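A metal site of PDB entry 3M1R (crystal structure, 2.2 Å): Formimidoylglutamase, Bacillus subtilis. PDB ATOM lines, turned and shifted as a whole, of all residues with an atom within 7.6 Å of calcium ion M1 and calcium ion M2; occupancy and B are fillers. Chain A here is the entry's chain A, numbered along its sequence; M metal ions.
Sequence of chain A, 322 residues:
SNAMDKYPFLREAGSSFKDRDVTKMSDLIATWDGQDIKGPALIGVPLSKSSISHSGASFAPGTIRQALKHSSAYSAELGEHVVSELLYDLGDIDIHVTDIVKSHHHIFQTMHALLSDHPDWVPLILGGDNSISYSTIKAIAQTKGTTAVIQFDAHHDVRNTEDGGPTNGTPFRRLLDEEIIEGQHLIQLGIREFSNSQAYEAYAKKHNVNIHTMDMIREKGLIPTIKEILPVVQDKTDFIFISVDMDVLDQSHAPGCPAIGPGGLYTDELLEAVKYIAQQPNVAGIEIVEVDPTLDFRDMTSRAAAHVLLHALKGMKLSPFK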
ATOM      1  N   ASP A 129      33.194  -4.090  -4.121  1.00  0.00           N
ATOM      2  CA  ASP A 129      32.655  -2.863  -3.558  1.00  0.00           C
ATOM      3  C   ASP A 129      32.324  -1.862  -4.652  1.00  0.00           C
ATOM      4  O   ASP A 129      32.505  -2.130  -5.838  1.00  0.00           O
ATOM      5  CB  ASP A 129      33.604  -2.270  -2.510  1.00  0.00           C
ATOM      6  CG  ASP A 129      34.900  -1.746  -3.104  1.00  0.00           C
ATOM      7  OD1 ASP A 129      35.963  -1.957  -2.476  1.00  0.00           O
ATOM      8  OD2 ASP A 129      34.866  -1.137  -4.194  1.00  0.00           O
ATOM      9  N   ASN A 130      31.833  -0.703  -4.232  1.00  0.00           N
ATOM     10  CA  ASN A 130      31.391   0.364  -5.126  1.00  0.00           C
ATOM     11  C   ASN A 130      32.386   0.796  -6.189  1.00  0.00           C
ATOM     12  O   ASN A 130      31.995   1.167  -7.300  1.00  0.00           O
ATOM     13  CB  ASN A 130      31.111   1.604  -4.299  1.00  0.00           C
ATOM     14  CG  ASN A 130      29.667   1.917  -4.228  1.00  0.00           C
ATOM     15  OD1 ASN A 130      29.205   2.395  -3.204  1.00  0.00           O
ATOM     16  ND2 ASN A 130      28.927   1.664  -5.315  1.00  0.00           N
ATOM     17  N   SER A 131      33.664   0.831  -5.830  1.00  0.00           N
ATOM     18  CA  SER A 131      34.652   1.469  -6.681  1.00  0.00           C
ATOM     19  C   SER A 131      34.779   0.744  -8.020  1.00  0.00           C
ATOM     20  O   SER A 131      35.307   1.313  -8.978  1.00  0.00           O
ATOM     21  CB  SER A 131      36.026   1.566  -5.989  1.00  0.00           C
ATOM     22  OG  SER A 131      36.552   0.278  -5.760  1.00  0.00           O
ATOM     23  N   SER A 133      32.549   0.282 -10.089  1.00  0.00           N
ATOM     24  CA  SER A 133      31.625   0.907 -11.058  1.00  0.00           C
ATOM     25  C   SER A 133      32.332   1.816 -12.076  1.00  0.00           C
ATOM     26  O   SER A 133      31.914   1.921 -13.237  1.00  0.00           O
ATOM     27  CB  SER A 133      30.545   1.696 -10.315  1.00  0.00           C
ATOM     28  OG  SER A 133      29.924   0.868  -9.352  1.00  0.00           O
ATOM     29  N   GLN A 151      21.575   4.250 -11.225  1.00  0.00           N
ATOM     30  CA  GLN A 151      22.199   3.807  -9.995  1.00  0.00           C
ATOM     31  C   GLN A 151      21.221   3.866  -8.829  1.00  0.00           C
ATOM     32  O   GLN A 151      20.697   4.939  -8.493  1.00  0.00           O
ATOM     33  CB  GLN A 151      23.509   4.563  -9.710  1.00  0.00           C
ATOM     34  CG  GLN A 151      23.343   5.997  -9.254  1.00  0.00           C
ATOM     35  CD  GLN A 151      24.625   6.579  -8.648  1.00  0.00           C
ATOM     36  OE1 GLN A 151      25.159   7.561  -9.136  1.00  0.00           O
ATOM     37  NE2 GLN A 151      25.106   5.964  -7.559  1.00  0.00           N
ATOM     38  N   PHE A 152      20.952   2.696  -8.267  1.00  0.00           N
ATOM     39  CA  PHE A 152      20.229   2.598  -7.012  1.00  0.00           C
ATOM     40  C   PHE A 152      21.251   2.782  -5.902  1.00  0.00           C
ATOM     41  O   PHE A 152      22.278   2.074  -5.875  1.00  0.00           O
ATOM     42  CB  PHE A 152      19.554   1.240  -6.864  1.00  0.00           C
ATOM     43  CG  PHE A 152      18.459   0.979  -7.859  1.00  0.00           C
ATOM     44  CD1 PHE A 152      17.144   1.302  -7.553  1.00  0.00           C
ATOM     45  CD2 PHE A 152      18.725   0.413  -9.072  1.00  0.00           C
ATOM     46  CE1 PHE A 152      16.116   1.063  -8.458  1.00  0.00           C
ATOM     47  CE2 PHE A 152      17.700   0.170  -9.999  1.00  0.00           C
ATOM     48  CZ  PHE A 152      16.410   0.500  -9.682  1.00  0.00           C
ATOM     49  N   ASP A 153      20.973   3.687  -4.974  1.00  0.00           N
ATOM     50  CA  ASP A 153      21.976   4.070  -3.999  1.00  0.00           C
ATOM     51  C   ASP A 153      21.414   5.070  -3.013  1.00  0.00           C
ATOM     52  O   ASP A 153      20.642   5.948  -3.369  1.00  0.00           O
ATOM     53  CB  ASP A 153      23.141   4.704  -4.740  1.00  0.00           C
ATOM     54  CG  ASP A 153      24.384   4.714  -3.920  1.00  0.00           C
ATOM     55  OD1 ASP A 153      24.270   4.736  -2.682  1.00  0.00           O
ATOM     56  OD2 ASP A 153      25.470   4.714  -4.514  1.00  0.00           O
ATOM     57  N   ALA A 154      21.808   4.918  -1.742  1.00  0.00           N
ATOM     58  CA  ALA A 154      21.517   5.931  -0.729  1.00  0.00           C
ATOM     59  C   ALA A 154      22.479   7.123  -0.873  1.00  0.00           C
ATOM     60  O   ALA A 154      22.148   8.239  -0.478  1.00  0.00           O
ATOM     61  CB  ALA A 154      21.621   5.316   0.688  1.00  0.00           C
ATOM     62  N   HIS A 155      23.653   6.876  -1.444  1.00  0.00           N
ATOM     63  CA  HIS A 155      24.722   7.891  -1.547  1.00  0.00           C
ATOM     64  C   HIS A 155      24.993   8.345  -2.984  1.00  0.00           C
ATOM     65  O   HIS A 155      24.809   7.580  -3.953  1.00  0.00           O
ATOM     66  CB  HIS A 155      26.022   7.343  -0.938  1.00  0.00           C
ATOM     67  CG  HIS A 155      25.798   6.646   0.370  1.00  0.00           C
ATOM     68  ND1 HIS A 155      25.699   5.278   0.459  1.00  0.00           N
ATOM     69  CD2 HIS A 155      25.611   7.121   1.612  1.00  0.00           C
ATOM     70  CE1 HIS A 155      25.485   4.929   1.724  1.00  0.00           C
ATOM     71  NE2 HIS A 155      25.432   6.033   2.447  1.00  0.00           N
ATOM     72  N   HIS A 156      25.427   9.590  -3.120  1.00  0.00           N
ATOM     73  CA  HIS A 156      25.680  10.124  -4.440  1.00  0.00           C
ATOM     74  C   HIS A 156      26.858   9.412  -5.052  1.00  0.00           C
ATOM     75  O   HIS A 156      26.921   9.241  -6.252  1.00  0.00           O
ATOM     76  CB  HIS A 156      25.962  11.627  -4.358  1.00  0.00           C
ATOM     77  CG  HIS A 156      24.748  12.455  -4.083  1.00  0.00           C
ATOM     78  ND1 HIS A 156      23.724  12.581  -4.989  1.00  0.00           N
ATOM     79  CD2 HIS A 156      24.426  13.232  -3.015  1.00  0.00           C
ATOM     80  CE1 HIS A 156      22.793  13.389  -4.484  1.00  0.00           C
ATOM     81  NE2 HIS A 156      23.196  13.796  -3.291  1.00  0.00           N
ATOM     82  N   ASP A 157      27.793   8.975  -4.204  1.00  0.00           N
ATOM     83  CA  ASP A 157      29.066   8.399  -4.647  1.00  0.00           C
ATOM     84  C   ASP A 157      29.885   9.324  -5.546  1.00  0.00           C
ATOM     85  O   ASP A 157      30.408   8.908  -6.588  1.00  0.00           O
ATOM     86  CB  ASP A 157      28.855   7.054  -5.349  1.00  0.00           C
ATOM     87  CG  ASP A 157      28.765   5.891  -4.350  1.00  0.00           C
ATOM     88  OD1 ASP A 157      28.169   6.079  -3.274  1.00  0.00           O
ATOM     89  OD2 ASP A 157      29.304   4.806  -4.655  1.00  0.00           O
ATOM     90  N   ASN A 168      36.356   4.467  -2.040  1.00  0.00           N
ATOM     91  CA  ASN A 168      35.117   3.701  -2.183  1.00  0.00           C
ATOM     92  C   ASN A 168      33.982   4.500  -2.811  1.00  0.00           C
ATOM     93  O   ASN A 168      33.280   3.996  -3.678  1.00  0.00           O
ATOM     94  CB  ASN A 168      34.660   3.037  -0.873  1.00  0.00           C
ATOM     95  CG  ASN A 168      33.688   1.903  -1.127  1.00  0.00           C
ATOM     96  OD1 ASN A 168      33.642   1.387  -2.259  1.00  0.00           O
ATOM     97  ND2 ASN A 168      32.910   1.527  -0.127  1.00  0.00           N
ATOM     98  N   GLY A 169      33.808   5.734  -2.364  1.00  0.00           N
ATOM     99  CA  GLY A 169      32.692   6.551  -2.806  1.00  0.00           C
ATOM    100  C   GLY A 169      33.051   7.536  -3.902  1.00  0.00           C
ATOM    101  O   GLY A 169      32.411   8.583  -4.012  1.00  0.00           O
ATOM    102  N   PRO A 171      33.481   6.548  -7.475  1.00  0.00           N
ATOM    103  CA  PRO A 171      33.310   6.120  -8.882  1.00  0.00           C
ATOM    104  C   PRO A 171      32.610   7.129  -9.785  1.00  0.00           C
ATOM    105  O   PRO A 171      33.068   7.351 -10.899  1.00  0.00           O
ATOM    106  CB  PRO A 171      32.484   4.846  -8.778  1.00  0.00           C
ATOM    107  CG  PRO A 171      31.870   4.873  -7.376  1.00  0.00           C
ATOM    108  CD  PRO A 171      32.915   5.572  -6.536  1.00  0.00           C
ATOM    109  N   PHE A 172      31.518   7.728  -9.318  1.00  0.00           N
ATOM    110  CA  PHE A 172      30.788   8.642 -10.195  1.00  0.00           C
ATOM    111  C   PHE A 172      31.400  10.024 -10.358  1.00  0.00           C
ATOM    112  O   PHE A 172      31.019  10.769 -11.266  1.00  0.00           O
ATOM    113  CB  PHE A 172      29.302   8.675  -9.845  1.00  0.00           C
ATOM    114  CG  PHE A 172      28.621   7.371 -10.063  1.00  0.00           C
ATOM    115  CD1 PHE A 172      28.467   6.472  -9.023  1.00  0.00           C
ATOM    116  CD2 PHE A 172      28.174   7.015 -11.319  1.00  0.00           C
ATOM    117  CE1 PHE A 172      27.852   5.257  -9.235  1.00  0.00           C
ATOM    118  CE2 PHE A 172      27.562   5.808 -11.545  1.00  0.00           C
ATOM    119  CZ  PHE A 172      27.400   4.920 -10.495  1.00  0.00           C
ATOM    120  N   ILE A 191      18.461   8.136  -3.100  1.00  0.00           N
ATOM    121  CA  ILE A 191      19.285   9.028  -2.307  1.00  0.00           C
ATOM    122  C   ILE A 191      18.600   9.409  -0.985  1.00  0.00           C
ATOM    123  O   ILE A 191      17.484   9.916  -0.979  1.00  0.00           O
ATOM    124  CB  ILE A 191      19.669  10.307  -3.084  1.00  0.00           C
ATOM    125  CG1 ILE A 191      20.478   9.933  -4.343  1.00  0.00           C
ATOM    126  CG2 ILE A 191      20.447  11.264  -2.169  1.00  0.00           C
ATOM    127  CD1 ILE A 191      21.859   9.349  -4.075  1.00  0.00           C
ATOM    128  N   SER A 195      22.371  10.690   4.515  1.00  0.00           N
ATOM    129  CA  SER A 195      23.387   9.800   3.978  1.00  0.00           C
ATOM    130  C   SER A 195      24.441  10.548   3.138  1.00  0.00           C
ATOM    131  O   SER A 195      25.402   9.952   2.675  1.00  0.00           O
ATOM    132  CB  SER A 195      22.747   8.661   3.150  1.00  0.00           C
ATOM    133  OG  SER A 195      22.298   7.606   3.979  1.00  0.00           O
ATOM    134  N   ASN A 196      24.264  11.862   2.970  1.00  0.00           N
ATOM    135  CA  ASN A 196      25.119  12.635   2.054  1.00  0.00           C
ATOM    136  C   ASN A 196      25.650  13.963   2.575  1.00  0.00           C
ATOM    137  O   ASN A 196      25.233  14.436   3.628  1.00  0.00           O
ATOM    138  CB  ASN A 196      24.378  12.891   0.742  1.00  0.00           C
ATOM    139  CG  ASN A 196      24.077  11.625   0.008  1.00  0.00           C
ATOM    140  OD1 ASN A 196      24.959  11.044  -0.617  1.00  0.00           O
ATOM    141  ND2 ASN A 196      22.846  11.142   0.138  1.00  0.00           N
ATOM    142  N   SER A 243      23.200  -0.002 -12.192  1.00  0.00           N
ATOM    143  CA  SER A 243      24.121  -0.168 -11.049  1.00  0.00           C
ATOM    144  C   SER A 243      23.323  -0.305  -9.753  1.00  0.00           C
ATOM    145  O   SER A 243      22.654   0.643  -9.308  1.00  0.00           O
ATOM    146  CB  SER A 243      25.111   0.987 -10.928  1.00  0.00           C
ATOM    147  OG  SER A 243      26.191   0.636 -10.070  1.00  0.00           O
ATOM    148  N   VAL A 244      23.362  -1.486  -9.162  1.00  0.00           N
ATOM    149  CA  VAL A 244      22.598  -1.692  -7.938  1.00  0.00           C
ATOM    150  C   VAL A 244      23.535  -1.673  -6.719  1.00  0.00           C
ATOM    151  O   VAL A 244      24.244  -2.647  -6.467  1.00  0.00           O
ATOM    152  CB  VAL A 244      21.820  -3.013  -7.971  1.00  0.00           C
ATOM    153  CG1 VAL A 244      21.227  -3.316  -6.576  1.00  0.00           C
ATOM    154  CG2 VAL A 244      20.724  -2.973  -9.026  1.00  0.00           C
ATOM    155  N   ASP A 245      23.543  -0.575  -5.984  1.00  0.00           N
ATOM    156  CA  ASP A 245      24.240  -0.574  -4.692  1.00  0.00           C
ATOM    157  C   ASP A 245      23.253  -1.045  -3.621  1.00  0.00           C
ATOM    158  O   ASP A 245      22.281  -0.349  -3.335  1.00  0.00           O
ATOM    159  CB  ASP A 245      24.777   0.811  -4.321  1.00  0.00           C
ATOM    160  CG  ASP A 245      25.376   0.844  -2.912  1.00  0.00           C
ATOM    161  OD1 ASP A 245      25.143  -0.084  -2.100  1.00  0.00           O
ATOM    162  OD2 ASP A 245      26.098   1.787  -2.612  1.00  0.00           O
ATOM    163  N   MET A 246      23.511  -2.212  -3.049  1.00  0.00           N
ATOM    164  CA  MET A 246      22.566  -2.852  -2.147  1.00  0.00           C
ATOM    165  C   MET A 246      22.255  -2.018  -0.901  1.00  0.00           C
ATOM    166  O   MET A 246      21.243  -2.259  -0.236  1.00  0.00           O
ATOM    167  CB  MET A 246      23.040  -4.264  -1.743  1.00  0.00           C
ATOM    168  CG  MET A 246      23.036  -5.289  -2.919  1.00  0.00           C
ATOM    169  SD  MET A 246      21.257  -5.549  -3.723  1.00  0.00           S
ATOM    170  CE  MET A 246      20.493  -6.826  -2.441  1.00  0.00           C
ATOM    171  N   ASP A 247      23.104  -1.053  -0.577  1.00  0.00           N
ATOM    172  CA  ASP A 247      22.836  -0.225   0.588  1.00  0.00           C
ATOM    173  C   ASP A 247      21.730   0.782   0.311  1.00  0.00           C
ATOM    174  O   ASP A 247      21.376   1.576   1.176  1.00  0.00           O
ATOM    175  CB  ASP A 247      24.126   0.441   1.136  1.00  0.00           C
ATOM    176  CG  ASP A 247      24.630   1.549   0.250  1.00  0.00           C
ATOM    177  OD1 ASP A 247      23.825   2.233  -0.437  1.00  0.00           O
ATOM    178  OD2 ASP A 247      25.858   1.767   0.260  1.00  0.00           O
ATOM    179  N   VAL A 248      21.160   0.742  -0.897  1.00  0.00           N
ATOM    180  CA  VAL A 248      19.954   1.501  -1.157  1.00  0.00           C
ATOM    181  C   VAL A 248      18.828   0.884  -0.314  1.00  0.00           C
ATOM    182  O   VAL A 248      17.842   1.530   0.002  1.00  0.00           O
ATOM    183  CB  VAL A 248      19.548   1.474  -2.650  1.00  0.00           C
ATOM    184  CG1 VAL A 248      18.903   0.132  -3.003  1.00  0.00           C
ATOM    185  CG2 VAL A 248      18.602   2.640  -2.986  1.00  0.00           C
ATOM    186  N   ALA A 259      27.336   0.243   4.801  1.00  0.00           N
ATOM    187  CA  ALA A 259      26.544   1.429   5.162  1.00  0.00           C
ATOM    188  C   ALA A 259      25.050   1.156   5.334  1.00  0.00           C
ATOM    189  O   ALA A 259      24.275   1.322   4.411  1.00  0.00           O
ATOM    190  CB  ALA A 259      26.747   2.570   4.138  1.00  0.00           C
ATOM    191  N   VAL A 289      26.749  -4.107  -6.074  1.00  0.00           N
ATOM    192  CA  VAL A 289      27.866  -3.784  -5.215  1.00  0.00           C
ATOM    193  C   VAL A 289      27.472  -3.695  -3.736  1.00  0.00           C
ATOM    194  O   VAL A 289      26.289  -3.692  -3.403  1.00  0.00           O
ATOM    195  CB  VAL A 289      28.532  -2.459  -5.636  1.00  0.00           C
ATOM    196  CG1 VAL A 289      29.008  -2.555  -7.078  1.00  0.00           C
ATOM    197  CG2 VAL A 289      27.546  -1.310  -5.467  1.00  0.00           C
ATOM    198  N   GLU A 290      28.486  -3.643  -2.874  1.00  0.00           N
ATOM    199  CA  GLU A 290      28.314  -3.382  -1.459  1.00  0.00           C
ATOM    200  C   GLU A 290      27.550  -4.465  -0.691  1.00  0.00           C
ATOM    201  O   GLU A 290      26.929  -4.178   0.334  1.00  0.00           O
ATOM    202  CB  GLU A 290      27.688  -1.998  -1.235  1.00  0.00           C
ATOM    203  CG  GLU A 290      28.568  -0.847  -1.778  1.00  0.00           C
ATOM    204  CD  GLU A 290      29.930  -0.759  -1.067  1.00  0.00           C
ATOM    205  OE1 GLU A 290      30.953  -0.548  -1.740  1.00  0.00           O
ATOM    206  OE2 GLU A 290      29.963  -0.934   0.169  1.00  0.00           O
HETATM  207 CA    CA M   1      27.230   3.339  -4.020  1.00  0.00          CA
HETATM  208 CA    CA M   2      25.770   3.583  -1.213  1.00  0.00          CA
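The backbone NH (N) of Asp 245 is in hydrogen-bond range of the backbone carbonyl oxygen (O) of Phe 152, 2.9 Å away. The backbone carbonyl oxygen of Asp 153 sits at hydrogen-bond distance from the backbone NH of Ile 191 (3.1 Å). The backbone NH of Asn 130 is in hydrogen-bond range of the side-chain carboxylate of Glu 290 (2.6 Å). The backbone NH (N) of Phe 172 sits at hydrogen-bond distance from the backbone carbonyl oxygen (O) of Asp 157 (3.2 Å). The side-chain amide nitrogen (NE2) of Gln 151 sits close to the side-chain carboxylate (OD2) of Asp 153, 3.3 Å away. O of Asn 130 is in hydrogen-bond range of OG of Ser 133 (2.9 Å). N of Asn 130 lies close to OD1 of Asn 168 (3.4 Å).
Within 4 Å of calcium ion M1: Asn 130, Asp 153, Asp 157 and Asp 245. The nearest printed residue that does not touch calcium ion M1 is Asp 247 (4.8 Å).
Of the 27 residues printed, 4 come within 4 Å of calcium ion M2. The nearest printed residue that does not touch calcium ion M2 is Asp 157 (4.03 Å).
The side-chain carboxylate (OD2) of Asp 153 binds calcium ion M1 (2.3 Å). The side-chain amide oxygen (OD1) of Asn 130 is bound to calcium ion M1. The side-chain carboxylate (OD2) of Asp 245 binds calcium ion M1, at 2.4 Å. OD2 of Asp 157 is bound to calcium ion M1, 2.6 Å away. ND2 of Asn 130 is bound to calcium ion M1 (2.7 Å). Slightly farther from calcium ion M1 lies OD1 of Asp 157 (3.0 Å).
Calcium ion M2 is bound by OD2 of Asp 245 (2.3 Å). OD2 of Asp 247 is bound to calcium ion M2, 2.3 Å away. Calcium ion M2 is bound by ND1 of His 155 (2.4 Å). Calcium ion M2 is bound by OD1 of Asp 153 (2.4 Å). OD1 of Asp 247 binds calcium ion M2, 2.5 Å away.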
